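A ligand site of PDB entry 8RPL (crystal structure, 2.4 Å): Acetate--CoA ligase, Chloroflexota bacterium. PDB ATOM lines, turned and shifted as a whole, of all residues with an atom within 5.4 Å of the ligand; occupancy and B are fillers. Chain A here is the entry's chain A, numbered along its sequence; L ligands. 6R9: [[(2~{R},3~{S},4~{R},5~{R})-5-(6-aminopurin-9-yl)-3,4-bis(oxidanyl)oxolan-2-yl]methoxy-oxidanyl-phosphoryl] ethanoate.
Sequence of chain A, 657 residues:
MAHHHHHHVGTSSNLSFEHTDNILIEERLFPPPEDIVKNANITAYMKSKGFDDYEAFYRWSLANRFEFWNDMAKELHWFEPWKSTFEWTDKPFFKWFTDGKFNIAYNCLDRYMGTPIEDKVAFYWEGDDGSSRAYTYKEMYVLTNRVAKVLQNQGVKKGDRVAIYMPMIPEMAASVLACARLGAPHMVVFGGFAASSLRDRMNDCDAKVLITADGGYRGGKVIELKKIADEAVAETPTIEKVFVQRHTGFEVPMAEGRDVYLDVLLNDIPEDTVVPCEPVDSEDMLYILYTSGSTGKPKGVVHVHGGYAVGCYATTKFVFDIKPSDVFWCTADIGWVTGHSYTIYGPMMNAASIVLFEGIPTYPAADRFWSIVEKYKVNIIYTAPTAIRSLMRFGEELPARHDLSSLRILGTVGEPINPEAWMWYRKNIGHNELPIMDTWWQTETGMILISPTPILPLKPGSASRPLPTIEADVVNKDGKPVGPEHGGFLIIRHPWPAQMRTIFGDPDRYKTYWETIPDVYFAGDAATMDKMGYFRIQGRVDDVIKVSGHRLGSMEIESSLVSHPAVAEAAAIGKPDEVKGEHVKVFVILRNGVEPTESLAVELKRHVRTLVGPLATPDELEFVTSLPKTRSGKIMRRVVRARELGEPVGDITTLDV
NE2 of Gln 442 lies within hydrogen-bond range of O26 of the ligand. An oxygen (O26) of the ligand is in hydrogen-bond range of the guanidinium group (NH1) of Arg 540 (2.9 Å). O06 of the ligand is in salt-bridge range of NZ of Lys 546 (3.2 Å). The backbone NH (N) of Thr 443 lies within hydrogen-bond range of an oxygen (O07) of the ligand, at 3.0 Å. A nitrogen (N24) of the ligand lies within hydrogen-bond range of the side-chain carboxylate (OD1) of Asp 438 (3.1 Å). A nitrogen (N24) of the ligand is in hydrogen-bond range of the backbone carbonyl oxygen (O) of Thr 439 (2.7 Å). NH1 of Arg 551 is in salt-bridge range of O07 of the ligand, at 2.8 Å. The side-chain carboxylate of Asp 525 is in hydrogen-bond range of an oxygen (O26) of the ligand, at 2.5 Å. N17 of the ligand lies within hydrogen-bond range of N of Gly 414, at 3.4 Å. An oxygen (O07) of the ligand is in hydrogen-bond range of the side-chain hydroxyl of Thr 443.
The backbone NH (N) of Thr 439 sits at hydrogen-bond distance from the backbone carbonyl oxygen (O) of Thr 412 (3.1 Å). The guanidinium group (NH1) of Arg 551 is in salt-bridge range of the side-chain carboxylate (OE1) of Glu 444. O of Ala 523 sits at hydrogen-bond distance from NE2 of Gln 442 (2.7 Å). The side-chain carboxylate (OD2) of Asp 525 lies within hydrogen-bond range of the indole nitrogen (NE1) of Trp 440 (2.9 Å). The side-chain amide nitrogen of Gln 442 lies close to the guanidinium group of Arg 540 (3.3 Å). OG1 of Thr 291 sits at hydrogen-bond distance from NE of Arg 551. The backbone carbonyl oxygen (O) of Ala 523 is in hydrogen-bond range of the guanidinium group (NH1) of Arg 540 (3.4 Å). The backbone carbonyl oxygen of Gly 414 is in hydrogen-bond range of the side-chain amino group of Lys 546, 2.9 Å away.
Val 337 touches the ligand. OG1 of Thr 338 touches C01 of the ligand, 3.8 Å away. CG2 of Val 413 touches C01 of the ligand, 3.97 Å away. C of Glu 415 touches C21 of the ligand, 3.4 Å away. Pro 416 touches the ligand (N to C21, 3.4 Å). N of Trp 440 touches N24 of the ligand, 3.6 Å away. O of Trp 441 touches C16 of the ligand, 3.5 Å away. Ile 537 touches the ligand (CB to C21, 3.7 Å). Hydrophobic or aromatic side chains within 4 Å of the ligand: Val 337, Val 413, Pro 416, Trp 440, Trp 441 and Ile 537.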
ATOM      1  N   THR A 291      16.611  -4.304   3.701  1.00  0.00           N
ATOM      2  CA  THR A 291      16.322  -3.203   2.832  1.00  0.00           C
ATOM      3  C   THR A 291      17.664  -2.628   2.367  1.00  0.00           C
ATOM      4  O   THR A 291      18.666  -2.696   3.072  1.00  0.00           O
ATOM      5  CB  THR A 291      15.481  -2.161   3.589  1.00  0.00           C
ATOM      6  OG1 THR A 291      15.147  -1.102   2.700  1.00  0.00           O
ATOM      7  CG2 THR A 291      16.278  -1.445   4.665  1.00  0.00           C
ATOM      8  N   VAL A 337       7.781  -4.639   2.793  1.00  0.00           N
ATOM      9  CA  VAL A 337       7.212  -4.142   4.037  1.00  0.00           C
ATOM     10  C   VAL A 337       5.698  -3.944   3.856  1.00  0.00           C
ATOM     11  O   VAL A 337       4.927  -4.183   4.755  1.00  0.00           O
ATOM     12  CB  VAL A 337       7.913  -2.865   4.528  1.00  0.00           C
ATOM     13  CG1 VAL A 337       7.701  -1.667   3.596  1.00  0.00           C
ATOM     14  CG2 VAL A 337       7.486  -2.540   5.958  1.00  0.00           C
ATOM     15  N   THR A 338       5.282  -3.561   2.650  1.00  0.00           N
ATOM     16  CA  THR A 338       3.898  -3.219   2.419  1.00  0.00           C
ATOM     17  C   THR A 338       3.030  -4.460   2.642  1.00  0.00           C
ATOM     18  O   THR A 338       1.912  -4.358   3.117  1.00  0.00           O
ATOM     19  CB  THR A 338       3.764  -2.662   1.005  1.00  0.00           C
ATOM     20  OG1 THR A 338       4.583  -1.505   0.895  1.00  0.00           O
ATOM     21  CG2 THR A 338       2.355  -2.190   0.704  1.00  0.00           C
ATOM     22  N   THR A 412      -2.460   3.983  -3.305  1.00  0.00           N
ATOM     23  CA  THR A 412      -1.213   3.823  -4.017  1.00  0.00           C
ATOM     24  C   THR A 412      -0.077   4.010  -3.028  1.00  0.00           C
ATOM     25  O   THR A 412      -0.204   4.762  -2.062  1.00  0.00           O
ATOM     26  CB  THR A 412      -1.159   4.771  -5.213  1.00  0.00           C
ATOM     27  OG1 THR A 412       0.110   4.565  -5.836  1.00  0.00           O
ATOM     28  CG2 THR A 412      -1.216   6.237  -4.803  1.00  0.00           C
ATOM     29  N   VAL A 413       1.031   3.311  -3.284  1.00  0.00           N
ATOM     30  CA  VAL A 413       2.200   3.341  -2.420  1.00  0.00           C
ATOM     31  C   VAL A 413       3.469   3.050  -3.199  1.00  0.00           C
ATOM     32  O   VAL A 413       3.481   2.294  -4.161  1.00  0.00           O
ATOM     33  CB  VAL A 413       2.042   2.288  -1.298  1.00  0.00           C
ATOM     34  CG1 VAL A 413       1.838   0.882  -1.862  1.00  0.00           C
ATOM     35  CG2 VAL A 413       3.203   2.304  -0.325  1.00  0.00           C
ATOM     36  N   GLY A 414       4.580   3.607  -2.723  1.00  0.00           N
ATOM     37  CA  GLY A 414       5.915   3.092  -2.993  1.00  0.00           C
ATOM     38  C   GLY A 414       6.744   4.067  -3.826  1.00  0.00           C
ATOM     39  O   GLY A 414       7.965   3.961  -3.820  1.00  0.00           O
ATOM     40  N   GLU A 415       6.077   5.026  -4.506  1.00  0.00           N
ATOM     41  CA  GLU A 415       6.733   5.895  -5.476  1.00  0.00           C
ATOM     42  C   GLU A 415       5.775   7.021  -5.839  1.00  0.00           C
ATOM     43  O   GLU A 415       4.590   6.930  -5.584  1.00  0.00           O
ATOM     44  CB  GLU A 415       7.202   5.126  -6.725  1.00  0.00           C
ATOM     45  CG  GLU A 415       6.140   4.201  -7.293  1.00  0.00           C
ATOM     46  CD  GLU A 415       6.511   3.096  -8.290  1.00  0.00           C
ATOM     47  OE1 GLU A 415       6.015   1.880  -8.164  1.00  0.00           O
ATOM     48  OE2 GLU A 415       7.243   3.531  -9.231  1.00  0.00           O
ATOM     49  N   PRO A 416       6.251   8.150  -6.399  1.00  0.00           N
ATOM     50  CA  PRO A 416       5.364   9.188  -6.933  1.00  0.00           C
ATOM     51  C   PRO A 416       4.439   8.587  -7.972  1.00  0.00           C
ATOM     52  O   PRO A 416       4.838   7.770  -8.809  1.00  0.00           O
ATOM     53  CB  PRO A 416       6.302  10.240  -7.576  1.00  0.00           C
ATOM     54  CG  PRO A 416       7.641   9.975  -6.899  1.00  0.00           C
ATOM     55  CD  PRO A 416       7.682   8.475  -6.622  1.00  0.00           C
ATOM     56  N   ASP A 438      -2.864   8.181  -1.367  1.00  0.00           N
ATOM     57  CA  ASP A 438      -1.449   8.182  -1.705  1.00  0.00           C
ATOM     58  C   ASP A 438      -0.574   8.201  -0.437  1.00  0.00           C
ATOM     59  O   ASP A 438      -0.283   9.255   0.120  1.00  0.00           O
ATOM     60  CB  ASP A 438      -1.179   9.371  -2.623  1.00  0.00           C
ATOM     61  CG  ASP A 438       0.242   9.429  -3.191  1.00  0.00           C
ATOM     62  OD1 ASP A 438       0.988   8.437  -2.991  1.00  0.00           O
ATOM     63  OD2 ASP A 438       0.584  10.456  -3.846  1.00  0.00           O
ATOM     64  N   THR A 439      -0.147   7.011   0.016  1.00  0.00           N
ATOM     65  CA  THR A 439       0.522   6.837   1.302  1.00  0.00           C
ATOM     66  C   THR A 439       2.047   6.917   1.179  1.00  0.00           C
ATOM     67  O   THR A 439       2.632   6.127   0.436  1.00  0.00           O
ATOM     68  CB  THR A 439       0.120   5.472   1.864  1.00  0.00           C
ATOM     69  OG1 THR A 439       0.712   4.427   1.074  1.00  0.00           O
ATOM     70  CG2 THR A 439      -1.396   5.329   1.972  1.00  0.00           C
ATOM     71  N   TRP A 440       2.669   7.844   1.919  1.00  0.00           N
ATOM     72  CA  TRP A 440       4.120   7.884   2.038  1.00  0.00           C
ATOM     73  C   TRP A 440       4.553   7.202   3.329  1.00  0.00           C
ATOM     74  O   TRP A 440       3.979   7.460   4.406  1.00  0.00           O
ATOM     75  CB  TRP A 440       4.668   9.318   1.978  1.00  0.00           C
ATOM     76  CG  TRP A 440       6.163   9.322   2.189  1.00  0.00           C
ATOM     77  CD1 TRP A 440       7.148   9.119   1.263  1.00  0.00           C
ATOM     78  CD2 TRP A 440       6.835   9.416   3.453  1.00  0.00           C
ATOM     79  NE1 TRP A 440       8.379   9.092   1.850  1.00  0.00           N
ATOM     80  CE2 TRP A 440       8.219   9.255   3.198  1.00  0.00           C
ATOM     81  CE3 TRP A 440       6.402   9.597   4.768  1.00  0.00           C
ATOM     82  CZ2 TRP A 440       9.164   9.289   4.218  1.00  0.00           C
ATOM     83  CZ3 TRP A 440       7.339   9.632   5.777  1.00  0.00           C
ATOM     84  CH2 TRP A 440       8.700   9.466   5.504  1.00  0.00           C
ATOM     85  N   TRP A 441       5.569   6.330   3.209  1.00  0.00           N
ATOM     86  CA  TRP A 441       6.277   5.689   4.316  1.00  0.00           C
ATOM     87  C   TRP A 441       7.439   4.857   3.773  1.00  0.00           C
ATOM     88  O   TRP A 441       7.783   4.999   2.613  1.00  0.00           O
ATOM     89  CB  TRP A 441       5.336   4.844   5.184  1.00  0.00           C
ATOM     90  CG  TRP A 441       4.611   3.726   4.475  1.00  0.00           C
ATOM     91  CD1 TRP A 441       3.693   3.836   3.468  1.00  0.00           C
ATOM     92  CD2 TRP A 441       4.694   2.324   4.791  1.00  0.00           C
ATOM     93  NE1 TRP A 441       3.200   2.602   3.133  1.00  0.00           N
ATOM     94  CE2 TRP A 441       3.806   1.656   3.925  1.00  0.00           C
ATOM     95  CE3 TRP A 441       5.411   1.576   5.718  1.00  0.00           C
ATOM     96  CZ2 TRP A 441       3.662   0.284   3.942  1.00  0.00           C
ATOM     97  CZ3 TRP A 441       5.247   0.209   5.749  1.00  0.00           C
ATOM     98  CH2 TRP A 441       4.374  -0.414   4.881  1.00  0.00           C
ATOM     99  N   GLN A 442       8.069   4.056   4.632  1.00  0.00           N
ATOM    100  CA  GLN A 442       9.281   3.330   4.295  1.00  0.00           C
ATOM    101  C   GLN A 442       9.364   2.086   5.163  1.00  0.00           C
ATOM    102  O   GLN A 442       8.736   2.018   6.202  1.00  0.00           O
ATOM    103  CB  GLN A 442      10.565   4.061   4.656  1.00  0.00           C
ATOM    104  CG  GLN A 442      10.488   5.578   4.509  1.00  0.00           C
ATOM    105  CD  GLN A 442      11.760   6.300   4.922  1.00  0.00           C
ATOM    106  OE1 GLN A 442      12.131   6.326   6.088  1.00  0.00           O
ATOM    107  NE2 GLN A 442      12.386   6.989   3.984  1.00  0.00           N
ATOM    108  N   THR A 443      10.224   1.147   4.772  1.00  0.00           N
ATOM    109  CA  THR A 443      10.468  -0.051   5.561  1.00  0.00           C
ATOM    110  C   THR A 443      10.790   0.344   7.009  1.00  0.00           C
ATOM    111  O   THR A 443      10.269  -0.249   7.960  1.00  0.00           O
ATOM    112  CB  THR A 443      11.601  -0.838   4.917  1.00  0.00           C
ATOM    113  OG1 THR A 443      11.228  -1.203   3.591  1.00  0.00           O
ATOM    114  CG2 THR A 443      11.840  -2.133   5.684  1.00  0.00           C
ATOM    115  N   GLU A 444      11.647   1.348   7.176  1.00  0.00           N
ATOM    116  CA  GLU A 444      12.114   1.765   8.487  1.00  0.00           C
ATOM    117  C   GLU A 444      10.962   2.307   9.355  1.00  0.00           C
ATOM    118  O   GLU A 444      11.105   2.325  10.568  1.00  0.00           O
ATOM    119  CB  GLU A 444      13.181   2.839   8.325  1.00  0.00           C
ATOM    120  CG  GLU A 444      14.458   2.355   7.620  1.00  0.00           C
ATOM    121  CD  GLU A 444      14.591   2.633   6.132  1.00  0.00           C
ATOM    122  OE1 GLU A 444      13.587   2.499   5.404  1.00  0.00           O
ATOM    123  OE2 GLU A 444      15.722   2.978   5.705  1.00  0.00           O
ATOM    124  N   ALA A 463       0.888  13.335  -1.177  1.00  0.00           N
ATOM    125  CA  ALA A 463       0.596  12.459  -0.057  1.00  0.00           C
ATOM    126  C   ALA A 463      -0.251  13.169   1.010  1.00  0.00           C
ATOM    127  O   ALA A 463      -0.631  12.517   1.965  1.00  0.00           O
ATOM    128  CB  ALA A 463       1.854  11.938   0.540  1.00  0.00           C
ATOM    129  N   ALA A 523      14.487  10.991   6.693  1.00  0.00           N
ATOM    130  CA  ALA A 523      13.888  10.002   5.826  1.00  0.00           C
ATOM    131  C   ALA A 523      14.762   9.666   4.625  1.00  0.00           C
ATOM    132  O   ALA A 523      14.597   8.604   4.032  1.00  0.00           O
ATOM    133  CB  ALA A 523      12.530  10.506   5.376  1.00  0.00           C
ATOM    134  N   ASP A 525      14.506  11.515   1.928  1.00  0.00           N
ATOM    135  CA  ASP A 525      13.635  11.961   0.843  1.00  0.00           C
ATOM    136  C   ASP A 525      13.637  13.477   0.787  1.00  0.00           C
ATOM    137  O   ASP A 525      13.688  14.143   1.827  1.00  0.00           O
ATOM    138  CB  ASP A 525      12.199  11.507   1.019  1.00  0.00           C
ATOM    139  CG  ASP A 525      11.906  10.082   0.561  1.00  0.00           C
ATOM    140  OD1 ASP A 525      12.346   9.745  -0.576  1.00  0.00           O
ATOM    141  OD2 ASP A 525      11.223   9.341   1.342  1.00  0.00           O
ATOM    142  N   ILE A 537       6.462  14.363  -2.186  1.00  0.00           N
ATOM    143  CA  ILE A 537       7.737  13.679  -2.101  1.00  0.00           C
ATOM    144  C   ILE A 537       8.387  13.576  -3.483  1.00  0.00           C
ATOM    145  O   ILE A 537       7.878  12.901  -4.365  1.00  0.00           O
ATOM    146  CB  ILE A 537       7.540  12.278  -1.501  1.00  0.00           C
ATOM    147  CG1 ILE A 537       6.511  12.253  -0.336  1.00  0.00           C
ATOM    148  CG2 ILE A 537       8.883  11.671  -1.093  1.00  0.00           C
ATOM    149  CD1 ILE A 537       6.824  13.171   0.811  1.00  0.00           C
ATOM    150  N   GLY A 539      11.844  12.603  -4.205  1.00  0.00           N
ATOM    151  CA  GLY A 539      12.506  11.315  -4.211  1.00  0.00           C
ATOM    152  C   GLY A 539      13.739  11.331  -3.324  1.00  0.00           C
ATOM    153  O   GLY A 539      14.006  12.298  -2.603  1.00  0.00           O
ATOM    154  N   ARG A 540      14.503  10.246  -3.412  1.00  0.00           N
ATOM    155  CA  ARG A 540      15.608   9.980  -2.502  1.00  0.00           C
ATOM    156  C   ARG A 540      16.717  11.001  -2.737  1.00  0.00           C
ATOM    157  O   ARG A 540      16.932  11.412  -3.860  1.00  0.00           O
ATOM    158  CB  ARG A 540      16.127   8.572  -2.761  1.00  0.00           C
ATOM    159  CG  ARG A 540      15.117   7.452  -2.517  1.00  0.00           C
ATOM    160  CD  ARG A 540      14.701   7.347  -1.073  1.00  0.00           C
ATOM    161  NE  ARG A 540      15.822   7.025  -0.199  1.00  0.00           N
ATOM    162  CZ  ARG A 540      15.709   6.566   1.051  1.00  0.00           C
ATOM    163  NH1 ARG A 540      14.534   6.231   1.535  1.00  0.00           N
ATOM    164  NH2 ARG A 540      16.789   6.431   1.797  1.00  0.00           N
ATOM    165  N   LYS A 546      14.634   3.166  -6.977  1.00  0.00           N
ATOM    166  CA  LYS A 546      13.427   2.358  -7.099  1.00  0.00           C
ATOM    167  C   LYS A 546      13.163   1.970  -8.553  1.00  0.00           C
ATOM    168  O   LYS A 546      12.998   2.834  -9.403  1.00  0.00           O
ATOM    169  CB  LYS A 546      12.172   3.104  -6.619  1.00  0.00           C
ATOM    170  CG  LYS A 546      11.896   3.079  -5.144  1.00  0.00           C
ATOM    171  CD  LYS A 546      10.760   2.154  -4.744  1.00  0.00           C
ATOM    172  CE  LYS A 546      10.597   2.326  -3.282  1.00  0.00           C
ATOM    173  NZ  LYS A 546       9.408   1.629  -2.786  1.00  0.00           N
ATOM    174  N   GLY A 549       8.936  -0.422  -8.542  1.00  0.00           N
ATOM    175  CA  GLY A 549       8.478  -0.535  -7.164  1.00  0.00           C
ATOM    176  C   GLY A 549       9.516  -1.059  -6.144  1.00  0.00           C
ATOM    177  O   GLY A 549       9.344  -0.902  -4.951  1.00  0.00           O
ATOM    178  N   ARG A 551      13.034  -1.378  -4.051  1.00  0.00           N
ATOM    179  CA  ARG A 551      14.127  -0.576  -3.530  1.00  0.00           C
ATOM    180  C   ARG A 551      15.461  -1.301  -3.694  1.00  0.00           C
ATOM    181  O   ARG A 551      15.646  -2.369  -3.116  1.00  0.00           O
ATOM    182  CB  ARG A 551      13.804  -0.293  -2.060  1.00  0.00           C
ATOM    183  CG  ARG A 551      14.862   0.481  -1.289  1.00  0.00           C
ATOM    184  CD  ARG A 551      14.257   0.990   0.007  1.00  0.00           C
ATOM    185  NE  ARG A 551      15.344   1.392   0.899  1.00  0.00           N
ATOM    186  CZ  ARG A 551      15.162   1.940   2.086  1.00  0.00           C
ATOM    187  NH1 ARG A 551      13.952   2.075   2.608  1.00  0.00           N
ATOM    188  NH2 ARG A 551      16.195   2.280   2.801  1.00  0.00           N
HETATM  189  C01 6R9 L   1       6.561   1.618   1.683  1.00  0.00           C
HETATM  190  C02 6R9 L   1       7.743   1.657   0.781  1.00  0.00           C
HETATM  191  C09 6R9 L   1      10.579   3.916   0.705  1.00  0.00           C
HETATM  192  C10 6R9 L   1      10.837   5.078  -0.212  1.00  0.00           C
HETATM  193  C11 6R9 L   1      10.599   6.457   0.385  1.00  0.00           C
HETATM  194  C12 6R9 L   1      10.343   7.276  -0.893  1.00  0.00           C
HETATM  195  C13 6R9 L   1       9.484   6.304  -1.699  1.00  0.00           C
HETATM  196  C16 6R9 L   1       7.241   5.627  -0.738  1.00  0.00           C
HETATM  197  C18 6R9 L   1       5.940   7.062  -1.580  1.00  0.00           C
HETATM  198  C19 6R9 L   1       7.205   7.372  -2.049  1.00  0.00           C
HETATM  199  C21 6R9 L   1       6.448   9.110  -3.181  1.00  0.00           C
HETATM  200  C23 6R9 L   1       4.875   7.889  -1.978  1.00  0.00           C
HETATM  201  N15 6R9 L   1       8.039   6.434  -1.496  1.00  0.00           N
HETATM  202  N17 6R9 L   1       5.970   5.941  -0.754  1.00  0.00           N
HETATM  203  N20 6R9 L   1       7.526   8.394  -2.871  1.00  0.00           N
HETATM  204  N22 6R9 L   1       5.176   8.952  -2.778  1.00  0.00           N
HETATM  205  N24 6R9 L   1       3.616   7.681  -1.575  1.00  0.00           N
HETATM  206  O03 6R9 L   1       7.700   1.956  -0.357  1.00  0.00           O
HETATM  207  O04 6R9 L   1       8.972   1.331   1.389  1.00  0.00           O
HETATM  208  O06 6R9 L   1      10.653   0.181  -0.166  1.00  0.00           O
HETATM  209  O07 6R9 L   1      11.441   1.135   1.979  1.00  0.00           O
HETATM  210  O08 6R9 L   1      10.776   2.682  -0.012  1.00  0.00           O
HETATM  211  O14 6R9 L   1       9.882   5.004  -1.278  1.00  0.00           O
HETATM  212  O25 6R9 L   1      11.462   7.536  -1.718  1.00  0.00           O
HETATM  213  O26 6R9 L   1      11.720   6.916   1.123  1.00  0.00           O
HETATM  214  P05 6R9 L   1      10.498   1.234   0.852  1.00  0.00           P
